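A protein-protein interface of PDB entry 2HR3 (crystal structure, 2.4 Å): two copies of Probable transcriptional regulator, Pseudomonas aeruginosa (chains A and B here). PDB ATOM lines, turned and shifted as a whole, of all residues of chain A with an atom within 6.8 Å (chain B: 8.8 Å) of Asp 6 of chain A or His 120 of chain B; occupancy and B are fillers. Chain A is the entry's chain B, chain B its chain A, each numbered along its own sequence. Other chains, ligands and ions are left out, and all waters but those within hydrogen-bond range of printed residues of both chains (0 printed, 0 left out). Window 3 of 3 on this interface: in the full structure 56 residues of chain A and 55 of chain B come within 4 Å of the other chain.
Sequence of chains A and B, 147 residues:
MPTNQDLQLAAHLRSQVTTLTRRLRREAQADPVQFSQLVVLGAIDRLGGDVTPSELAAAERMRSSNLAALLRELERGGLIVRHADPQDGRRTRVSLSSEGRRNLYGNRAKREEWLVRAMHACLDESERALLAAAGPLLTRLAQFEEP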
ATOM      1  N   THR A   3     -34.589  23.543   0.456  1.00  0.00           N
ATOM      2  CA  THR A   3     -33.632  24.656   0.485  1.00  0.00           C
ATOM      3  C   THR A   3     -32.887  24.650   1.813  1.00  0.00           C
ATOM      4  O   THR A   3     -31.842  25.257   1.915  1.00  0.00           O
ATOM      5  CB  THR A   3     -34.274  26.111   0.211  1.00  0.00           C
ATOM      6  OG1 THR A   3     -35.592  26.202   0.754  1.00  0.00           O
ATOM      7  CG2 THR A   3     -34.328  26.486  -1.308  1.00  0.00           C
ATOM      8  N   ASN A   4     -33.404  23.958   2.824  1.00  0.00           N
ATOM      9  CA  ASN A   4     -32.665  23.817   4.090  1.00  0.00           C
ATOM     10  C   ASN A   4     -31.212  23.375   3.900  1.00  0.00           C
ATOM     11  O   ASN A   4     -30.289  24.071   4.371  1.00  0.00           O
ATOM     12  CB  ASN A   4     -33.357  22.833   5.023  1.00  0.00           C
ATOM     13  CG  ASN A   4     -32.792  22.881   6.430  1.00  0.00           C
ATOM     14  OD1 ASN A   4     -31.761  23.533   6.700  1.00  0.00           O
ATOM     15  ND2 ASN A   4     -33.485  22.205   7.351  1.00  0.00           N
ATOM     16  N   GLN A   5     -31.000  22.239   3.216  1.00  0.00           N
ATOM     17  CA  GLN A   5     -29.643  21.867   2.782  1.00  0.00           C
ATOM     18  C   GLN A   5     -29.034  22.956   1.902  1.00  0.00           C
ATOM     19  O   GLN A   5     -27.872  23.329   2.079  1.00  0.00           O
ATOM     20  CB  GLN A   5     -29.642  20.527   2.046  1.00  0.00           C
ATOM     21  N   ASP A   6     -29.835  23.484   0.973  1.00  0.00           N
ATOM     22  CA  ASP A   6     -29.348  24.469  -0.006  1.00  0.00           C
ATOM     23  C   ASP A   6     -28.753  25.690   0.638  1.00  0.00           C
ATOM     24  O   ASP A   6     -27.671  26.097   0.300  1.00  0.00           O
ATOM     25  CB  ASP A   6     -30.476  24.942  -0.946  1.00  0.00           C
ATOM     26  CG  ASP A   6     -30.866  23.916  -1.992  1.00  0.00           C
ATOM     27  OD1 ASP A   6     -30.027  23.038  -2.286  1.00  0.00           O
ATOM     28  OD2 ASP A   6     -32.005  24.032  -2.532  1.00  0.00           O
ATOM     29  N   LEU A   7     -29.528  26.279   1.520  1.00  0.00           N
ATOM     30  CA  LEU A   7     -29.135  27.365   2.427  1.00  0.00           C
ATOM     31  C   LEU A   7     -27.912  27.050   3.334  1.00  0.00           C
ATOM     32  O   LEU A   7     -26.997  27.820   3.385  1.00  0.00           O
ATOM     33  CB  LEU A   7     -30.377  27.750   3.304  1.00  0.00           C
ATOM     34  CG  LEU A   7     -31.400  28.582   2.530  1.00  0.00           C
ATOM     35  CD1 LEU A   7     -32.711  28.593   3.184  1.00  0.00           C
ATOM     36  CD2 LEU A   7     -30.800  30.011   2.327  1.00  0.00           C
ATOM     37  N   GLN A   8     -27.926  25.916   4.020  1.00  0.00           N
ATOM     38  CA  GLN A   8     -26.701  25.332   4.638  1.00  0.00           C
ATOM     39  C   GLN A   8     -25.458  25.380   3.729  1.00  0.00           C
ATOM     40  O   GLN A   8     -24.428  25.897   4.137  1.00  0.00           O
ATOM     41  CB  GLN A   8     -26.949  23.856   5.068  1.00  0.00           C
ATOM     42  CG  GLN A   8     -27.240  23.574   6.568  1.00  0.00           C
ATOM     43  N   LEU A   9     -25.585  24.886   2.494  1.00  0.00           N
ATOM     44  CA  LEU A   9     -24.461  24.802   1.557  1.00  0.00           C
ATOM     45  C   LEU A   9     -23.952  26.174   1.166  1.00  0.00           C
ATOM     46  O   LEU A   9     -22.739  26.437   1.172  1.00  0.00           O
ATOM     47  CB  LEU A   9     -24.901  24.106   0.251  1.00  0.00           C
ATOM     48  CG  LEU A   9     -23.804  23.380  -0.546  1.00  0.00           C
ATOM     49  CD1 LEU A   9     -24.280  23.160  -2.024  1.00  0.00           C
ATOM     50  CD2 LEU A   9     -22.343  23.879  -0.497  1.00  0.00           C
ATOM     51  N   ALA A  10     -24.892  27.053   0.814  1.00  0.00           N
ATOM     52  CA  ALA A  10     -24.577  28.418   0.429  1.00  0.00           C
ATOM     53  C   ALA A  10     -23.975  29.253   1.571  1.00  0.00           C
ATOM     54  O   ALA A  10     -23.107  30.025   1.343  1.00  0.00           O
ATOM     55  CB  ALA A  10     -25.805  29.106  -0.116  1.00  0.00           C
ATOM     56  N   ALA A  11     -24.432  29.077   2.789  1.00  0.00           N
ATOM     57  CA  ALA A  11     -23.856  29.825   3.924  1.00  0.00           C
ATOM     58  C   ALA A  11     -22.441  29.351   4.216  1.00  0.00           C
ATOM     59  O   ALA A  11     -21.552  30.174   4.490  1.00  0.00           O
ATOM     60  CB  ALA A  11     -24.720  29.611   5.171  1.00  0.00           C
ATOM     61  N   LEU A 141     -20.045  30.188 -10.754  1.00  0.00           N
ATOM     62  CA  LEU A 141     -20.989  30.860  -9.875  1.00  0.00           C
ATOM     63  C   LEU A 141     -20.724  32.366  -9.883  1.00  0.00           C
ATOM     64  O   LEU A 141     -21.685  33.157  -9.784  1.00  0.00           O
ATOM     65  CB  LEU A 141     -20.916  30.322  -8.477  1.00  0.00           C
ATOM     66  CG  LEU A 141     -21.235  28.861  -8.286  1.00  0.00           C
ATOM     67  CD1 LEU A 141     -20.707  28.439  -6.873  1.00  0.00           C
ATOM     68  CD2 LEU A 141     -22.749  28.652  -8.436  1.00  0.00           C
ATOM     69  N   GLU B 112     -26.547  34.933   0.271  1.00  0.00           N
ATOM     70  CA  GLU B 112     -26.733  33.514   0.362  1.00  0.00           C
ATOM     71  C   GLU B 112     -27.910  33.024  -0.469  1.00  0.00           C
ATOM     72  O   GLU B 112     -27.852  31.940  -1.075  1.00  0.00           O
ATOM     73  CB  GLU B 112     -26.894  33.096   1.830  1.00  0.00           C
ATOM     74  CG  GLU B 112     -25.542  33.050   2.510  1.00  0.00           C
ATOM     75  CD  GLU B 112     -25.609  33.031   4.018  1.00  0.00           C
ATOM     76  OE1 GLU B 112     -26.649  32.644   4.592  1.00  0.00           O
ATOM     77  OE2 GLU B 112     -24.610  33.438   4.633  1.00  0.00           O
ATOM     78  N   GLU B 113     -28.982  33.805  -0.438  1.00  0.00           N
ATOM     79  CA  GLU B 113     -30.124  33.576  -1.329  1.00  0.00           C
ATOM     80  C   GLU B 113     -29.655  33.673  -2.776  1.00  0.00           C
ATOM     81  O   GLU B 113     -29.823  32.744  -3.517  1.00  0.00           O
ATOM     82  CB  GLU B 113     -31.245  34.586  -1.042  1.00  0.00           C
ATOM     83  CG  GLU B 113     -32.064  34.298   0.200  1.00  0.00           C
ATOM     84  CD  GLU B 113     -32.619  35.565   0.772  1.00  0.00           C
ATOM     85  OE1 GLU B 113     -33.184  36.345  -0.041  1.00  0.00           O
ATOM     86  OE2 GLU B 113     -32.461  35.814   2.004  1.00  0.00           O
ATOM     87  N   TRP B 114     -29.051  34.796  -3.154  1.00  0.00           N
ATOM     88  CA  TRP B 114     -28.324  34.894  -4.393  1.00  0.00           C
ATOM     89  C   TRP B 114     -27.579  33.588  -4.753  1.00  0.00           C
ATOM     90  O   TRP B 114     -27.782  33.069  -5.804  1.00  0.00           O
ATOM     91  CB  TRP B 114     -27.336  36.074  -4.427  1.00  0.00           C
ATOM     92  CG  TRP B 114     -26.664  36.102  -5.780  1.00  0.00           C
ATOM     93  CD1 TRP B 114     -27.215  36.572  -6.936  1.00  0.00           C
ATOM     94  CD2 TRP B 114     -25.395  35.566  -6.143  1.00  0.00           C
ATOM     95  NE1 TRP B 114     -26.370  36.368  -7.998  1.00  0.00           N
ATOM     96  CE2 TRP B 114     -25.250  35.729  -7.540  1.00  0.00           C
ATOM     97  CE3 TRP B 114     -24.399  34.897  -5.450  1.00  0.00           C
ATOM     98  CZ2 TRP B 114     -24.124  35.295  -8.233  1.00  0.00           C
ATOM     99  CZ3 TRP B 114     -23.267  34.451  -6.160  1.00  0.00           C
ATOM    100  CH2 TRP B 114     -23.127  34.677  -7.501  1.00  0.00           C
ATOM    101  N   LEU B 115     -26.715  33.077  -3.872  1.00  0.00           N
ATOM    102  CA  LEU B 115     -25.791  31.939  -4.194  1.00  0.00           C
ATOM    103  C   LEU B 115     -26.497  30.664  -4.444  1.00  0.00           C
ATOM    104  O   LEU B 115     -26.073  29.877  -5.285  1.00  0.00           O
ATOM    105  CB  LEU B 115     -24.865  31.649  -3.035  1.00  0.00           C
ATOM    106  CG  LEU B 115     -23.370  31.543  -3.319  1.00  0.00           C
ATOM    107  CD1 LEU B 115     -22.701  31.105  -1.973  1.00  0.00           C
ATOM    108  CD2 LEU B 115     -22.987  30.646  -4.469  1.00  0.00           C
ATOM    109  N   VAL B 116     -27.534  30.431  -3.642  1.00  0.00           N
ATOM    110  CA  VAL B 116     -28.483  29.314  -3.848  1.00  0.00           C
ATOM    111  C   VAL B 116     -29.077  29.305  -5.236  1.00  0.00           C
ATOM    112  O   VAL B 116     -29.203  28.240  -5.871  1.00  0.00           O
ATOM    113  CB  VAL B 116     -29.665  29.335  -2.797  1.00  0.00           C
ATOM    114  CG1 VAL B 116     -30.736  28.315  -3.135  1.00  0.00           C
ATOM    115  CG2 VAL B 116     -29.132  29.065  -1.367  1.00  0.00           C
ATOM    116  N   ARG B 117     -29.483  30.483  -5.688  1.00  0.00           N
ATOM    117  CA  ARG B 117     -30.024  30.667  -7.031  1.00  0.00           C
ATOM    118  C   ARG B 117     -28.974  30.512  -8.099  1.00  0.00           C
ATOM    119  O   ARG B 117     -29.279  29.969  -9.147  1.00  0.00           O
ATOM    120  CB  ARG B 117     -30.677  32.037  -7.183  1.00  0.00           C
ATOM    121  CG  ARG B 117     -32.123  32.082  -6.754  1.00  0.00           C
ATOM    122  CD  ARG B 117     -32.791  33.471  -6.932  1.00  0.00           C
ATOM    123  NE  ARG B 117     -31.894  34.643  -6.807  1.00  0.00           N
ATOM    124  CZ  ARG B 117     -31.385  35.317  -7.854  1.00  0.00           C
ATOM    125  NH1 ARG B 117     -31.657  34.951  -9.133  1.00  0.00           N
ATOM    126  NH2 ARG B 117     -30.586  36.366  -7.641  1.00  0.00           N
ATOM    127  N   ALA B 118     -27.757  31.007  -7.887  1.00  0.00           N
ATOM    128  CA  ALA B 118     -26.587  30.599  -8.778  1.00  0.00           C
ATOM    129  C   ALA B 118     -26.403  29.092  -8.898  1.00  0.00           C
ATOM    130  O   ALA B 118     -26.262  28.555  -9.970  1.00  0.00           O
ATOM    131  CB  ALA B 118     -25.226  31.197  -8.276  1.00  0.00           C
ATOM    132  N   MET B 119     -26.397  28.439  -7.753  1.00  0.00           N
ATOM    133  CA  MET B 119     -26.116  27.053  -7.657  1.00  0.00           C
ATOM    134  C   MET B 119     -27.195  26.222  -8.249  1.00  0.00           C
ATOM    135  O   MET B 119     -26.933  25.152  -8.733  1.00  0.00           O
ATOM    136  CB  MET B 119     -25.961  26.700  -6.216  1.00  0.00           C
ATOM    137  CG  MET B 119     -24.591  27.102  -5.661  1.00  0.00           C
ATOM    138  SD  MET B 119     -24.282  26.629  -3.727  1.00  0.00           S
ATOM    139  CE  MET B 119     -23.316  25.105  -4.062  1.00  0.00           C
ATOM    140  N   HIS B 120     -28.434  26.725  -8.283  1.00  0.00           N
ATOM    141  CA  HIS B 120     -29.492  25.959  -8.914  1.00  0.00           C
ATOM    142  C   HIS B 120     -29.523  26.155 -10.379  1.00  0.00           C
ATOM    143  O   HIS B 120     -29.986  25.283 -11.106  1.00  0.00           O
ATOM    144  CB  HIS B 120     -30.826  26.160  -8.217  1.00  0.00           C
ATOM    145  CG  HIS B 120     -30.960  25.249  -7.044  1.00  0.00           C
ATOM    146  ND1 HIS B 120     -31.614  24.041  -7.116  1.00  0.00           N
ATOM    147  CD2 HIS B 120     -30.359  25.276  -5.828  1.00  0.00           C
ATOM    148  CE1 HIS B 120     -31.508  23.413  -5.960  1.00  0.00           C
ATOM    149  NE2 HIS B 120     -30.736  24.132  -5.168  1.00  0.00           N
ATOM    150  N   ALA B 121     -28.957  27.260 -10.818  1.00  0.00           N
ATOM    151  CA  ALA B 121     -28.982  27.621 -12.238  1.00  0.00           C
ATOM    152  C   ALA B 121     -27.692  27.194 -12.987  1.00  0.00           C
ATOM    153  O   ALA B 121     -27.686  27.157 -14.178  1.00  0.00           O
ATOM    154  CB  ALA B 121     -29.176  29.151 -12.345  1.00  0.00           C
ATOM    155  N   CYS B 122     -26.604  26.962 -12.277  1.00  0.00           N
ATOM    156  CA  CYS B 122     -25.247  26.814 -12.860  1.00  0.00           C
ATOM    157  C   CYS B 122     -24.694  25.387 -12.772  1.00  0.00           C
ATOM    158  O   CYS B 122     -23.792  25.028 -13.530  1.00  0.00           O
ATOM    159  CB  CYS B 122     -24.227  27.721 -12.080  1.00  0.00           C
ATOM    160  SG  CYS B 122     -24.553  29.463 -12.371  1.00  0.00           S
ATOM    161  N   LEU B 123     -25.257  24.603 -11.848  1.00  0.00           N
ATOM    162  CA  LEU B 123     -24.681  23.393 -11.377  1.00  0.00           C
ATOM    163  C   LEU B 123     -25.765  22.382 -11.229  1.00  0.00           C
ATOM    164  O   LEU B 123     -26.844  22.764 -10.837  1.00  0.00           O
ATOM    165  CB  LEU B 123     -24.064  23.620  -9.921  1.00  0.00           C
ATOM    166  CG  LEU B 123     -23.126  24.790  -9.503  1.00  0.00           C
ATOM    167  CD1 LEU B 123     -22.842  24.810  -7.940  1.00  0.00           C
ATOM    168  CD2 LEU B 123     -21.828  24.801 -10.268  1.00  0.00           C
ATOM    169  N   ASP B 124     -25.457  21.092 -11.410  1.00  0.00           N
ATOM    170  CA  ASP B 124     -26.363  20.023 -10.941  1.00  0.00           C
ATOM    171  C   ASP B 124     -26.064  19.548  -9.523  1.00  0.00           C
ATOM    172  O   ASP B 124     -25.163  20.030  -8.892  1.00  0.00           O
ATOM    173  CB  ASP B 124     -26.435  18.829 -11.924  1.00  0.00           C
ATOM    174  CG  ASP B 124     -25.117  18.034 -12.052  1.00  0.00           C
ATOM    175  OD1 ASP B 124     -24.170  18.211 -11.268  1.00  0.00           O
ATOM    176  OD2 ASP B 124     -25.016  17.215 -13.005  1.00  0.00           O
ATOM    177  N   GLU B 125     -26.824  18.580  -9.073  1.00  0.00           N
ATOM    178  CA  GLU B 125     -26.773  18.033  -7.725  1.00  0.00           C
ATOM    179  C   GLU B 125     -25.388  17.458  -7.326  1.00  0.00           C
ATOM    180  O   GLU B 125     -24.879  17.696  -6.176  1.00  0.00           O
ATOM    181  CB  GLU B 125     -27.915  16.997  -7.605  1.00  0.00           C
ATOM    182  CG  GLU B 125     -28.318  16.488  -6.204  1.00  0.00           C
ATOM    183  N   GLU B 127     -22.601  18.266  -8.664  1.00  0.00           N
ATOM    184  CA  GLU B 127     -21.679  19.382  -8.596  1.00  0.00           C
ATOM    185  C   GLU B 127     -21.761  20.200  -7.313  1.00  0.00           C
ATOM    186  O   GLU B 127     -20.765  20.715  -6.864  1.00  0.00           O
ATOM    187  CB  GLU B 127     -21.929  20.289  -9.774  1.00  0.00           C
ATOM    188  CG  GLU B 127     -21.348  19.741 -11.081  1.00  0.00           C
ATOM    189  CD  GLU B 127     -21.794  20.554 -12.289  1.00  0.00           C
ATOM    190  OE1 GLU B 127     -22.802  21.258 -12.210  1.00  0.00           O
ATOM    191  OE2 GLU B 127     -21.115  20.527 -13.303  1.00  0.00           O
ATOM    192  N   ARG B 128     -22.972  20.410  -6.791  1.00  0.00           N
ATOM    193  CA  ARG B 128     -23.137  20.962  -5.423  1.00  0.00           C
ATOM    194  C   ARG B 128     -22.536  20.070  -4.327  1.00  0.00           C
ATOM    195  O   ARG B 128     -22.150  20.555  -3.261  1.00  0.00           O
ATOM    196  CB  ARG B 128     -24.598  21.101  -5.113  1.00  0.00           C
ATOM    197  CG  ARG B 128     -25.272  22.148  -5.895  1.00  0.00           C
ATOM    198  CD  ARG B 128     -26.764  22.191  -5.547  1.00  0.00           C
ATOM    199  NE  ARG B 128     -27.347  22.556  -6.789  1.00  0.00           N
ATOM    200  CZ  ARG B 128     -28.156  21.839  -7.555  1.00  0.00           C
ATOM    201  NH1 ARG B 128     -28.702  20.688  -7.194  1.00  0.00           N
ATOM    202  NH2 ARG B 128     -28.486  22.392  -8.691  1.00  0.00           N
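A ring nitrogen (NE2) of His 120 of chain B sits at hydrogen-bond distance from the side-chain carboxylate (OD2) of Asp 6 of chain A (2.9 Å).
The side-chain sulfur of Cys 122 of chain B sits close to the backbone carbonyl oxygen of Ala 118 of chain B (3.1 Å).
The backbone carbonyl oxygen of Met 119 of chain B sits at hydrogen-bond distance from the guanidinium group of Arg 128 of chain B.
O of Leu 123 of chain B lies within hydrogen-bond range of NH2 of Arg 128 of chain B.
Among the printed residues, merely in contact across the chains: Asp 6 of chain A with Val 116 of chain B (3.7 Å), Leu 9 of chain A with Met 119 of chain B (3.0 Å), Leu 9 of chain A with Arg 128 of chain B (3.6 Å), Ala 10 of chain A with Glu 112 of chain B (3.6 Å), Ala 10 of chain A with Leu 115 of chain B (3.5 Å), Ala 10 of chain A with Val 116 of chain B (3.6 Å), Ala 11 of chain A with Glu 112 of chain B (3.6 Å), Leu 141 of chain A with Trp 114 of chain B (3.1 Å), Leu 141 of chain A with Leu 115 of chain B (3.98 Å), Leu 141 of chain A with Ala 118 of chain B (3.6 Å), Leu 141 of chain A with Met 119 of chain B (3.7 Å) and Leu 141 of chain A with Leu 123 of chain B (3.9 Å).
Asp 6 of chain A touches just these residues of chain B: Val 116 and His 120.
Of chain A, only Asp 6 (2.9 Å) comes within 4 Å of His 120 of chain B.
Of the printed residues of chain A, Leu 115 of chain B touches Ala 10 and Leu 141.
Of the printed residues of chain B, Leu 141 of chain A touches Trp 114 (3.1 Å), Leu 115 (3.98 Å), Ala 118 (3.6 Å), Met 119 (3.7 Å) and Leu 123 (3.9 Å).
Printed residues of chain A within 4 Å of Ala 118 of chain B: Leu 141.
Of the printed residues of chain B, Leu 9 of chain A touches Met 119 and Arg 128.
Cys 122 of chain B touches none of the printed residues of chain A.
Ala 121 of chain B touches none of the printed residues of chain A.
The nearest residue of chain A that does not touch His 120 of chain B is Thr 3 of chain A (5.8 Å).
Of the 16 printed residues of chain B, 9 touch a printed residue of chain A.
Along chain B the printed residues that touch a printed residue of chain A span positions 112 to 128.
Of the 10 printed residues of chain A, 5 touch a printed residue of chain B.
Hydrophobic or aromatic side chains of chain A that line the printed part of chain B: Leu 9, Ala 10, Ala 11 and Leu 141.
Among the printed residues, no Asp or Glu carboxylate lies within 4 Å of a Lys or Arg side-chain nitrogen of the other chain.
No position is printed for both chains.
Of the 13 pairs that touch across the chains among the printed residues, none has its exchanged pair printed and touching as well.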
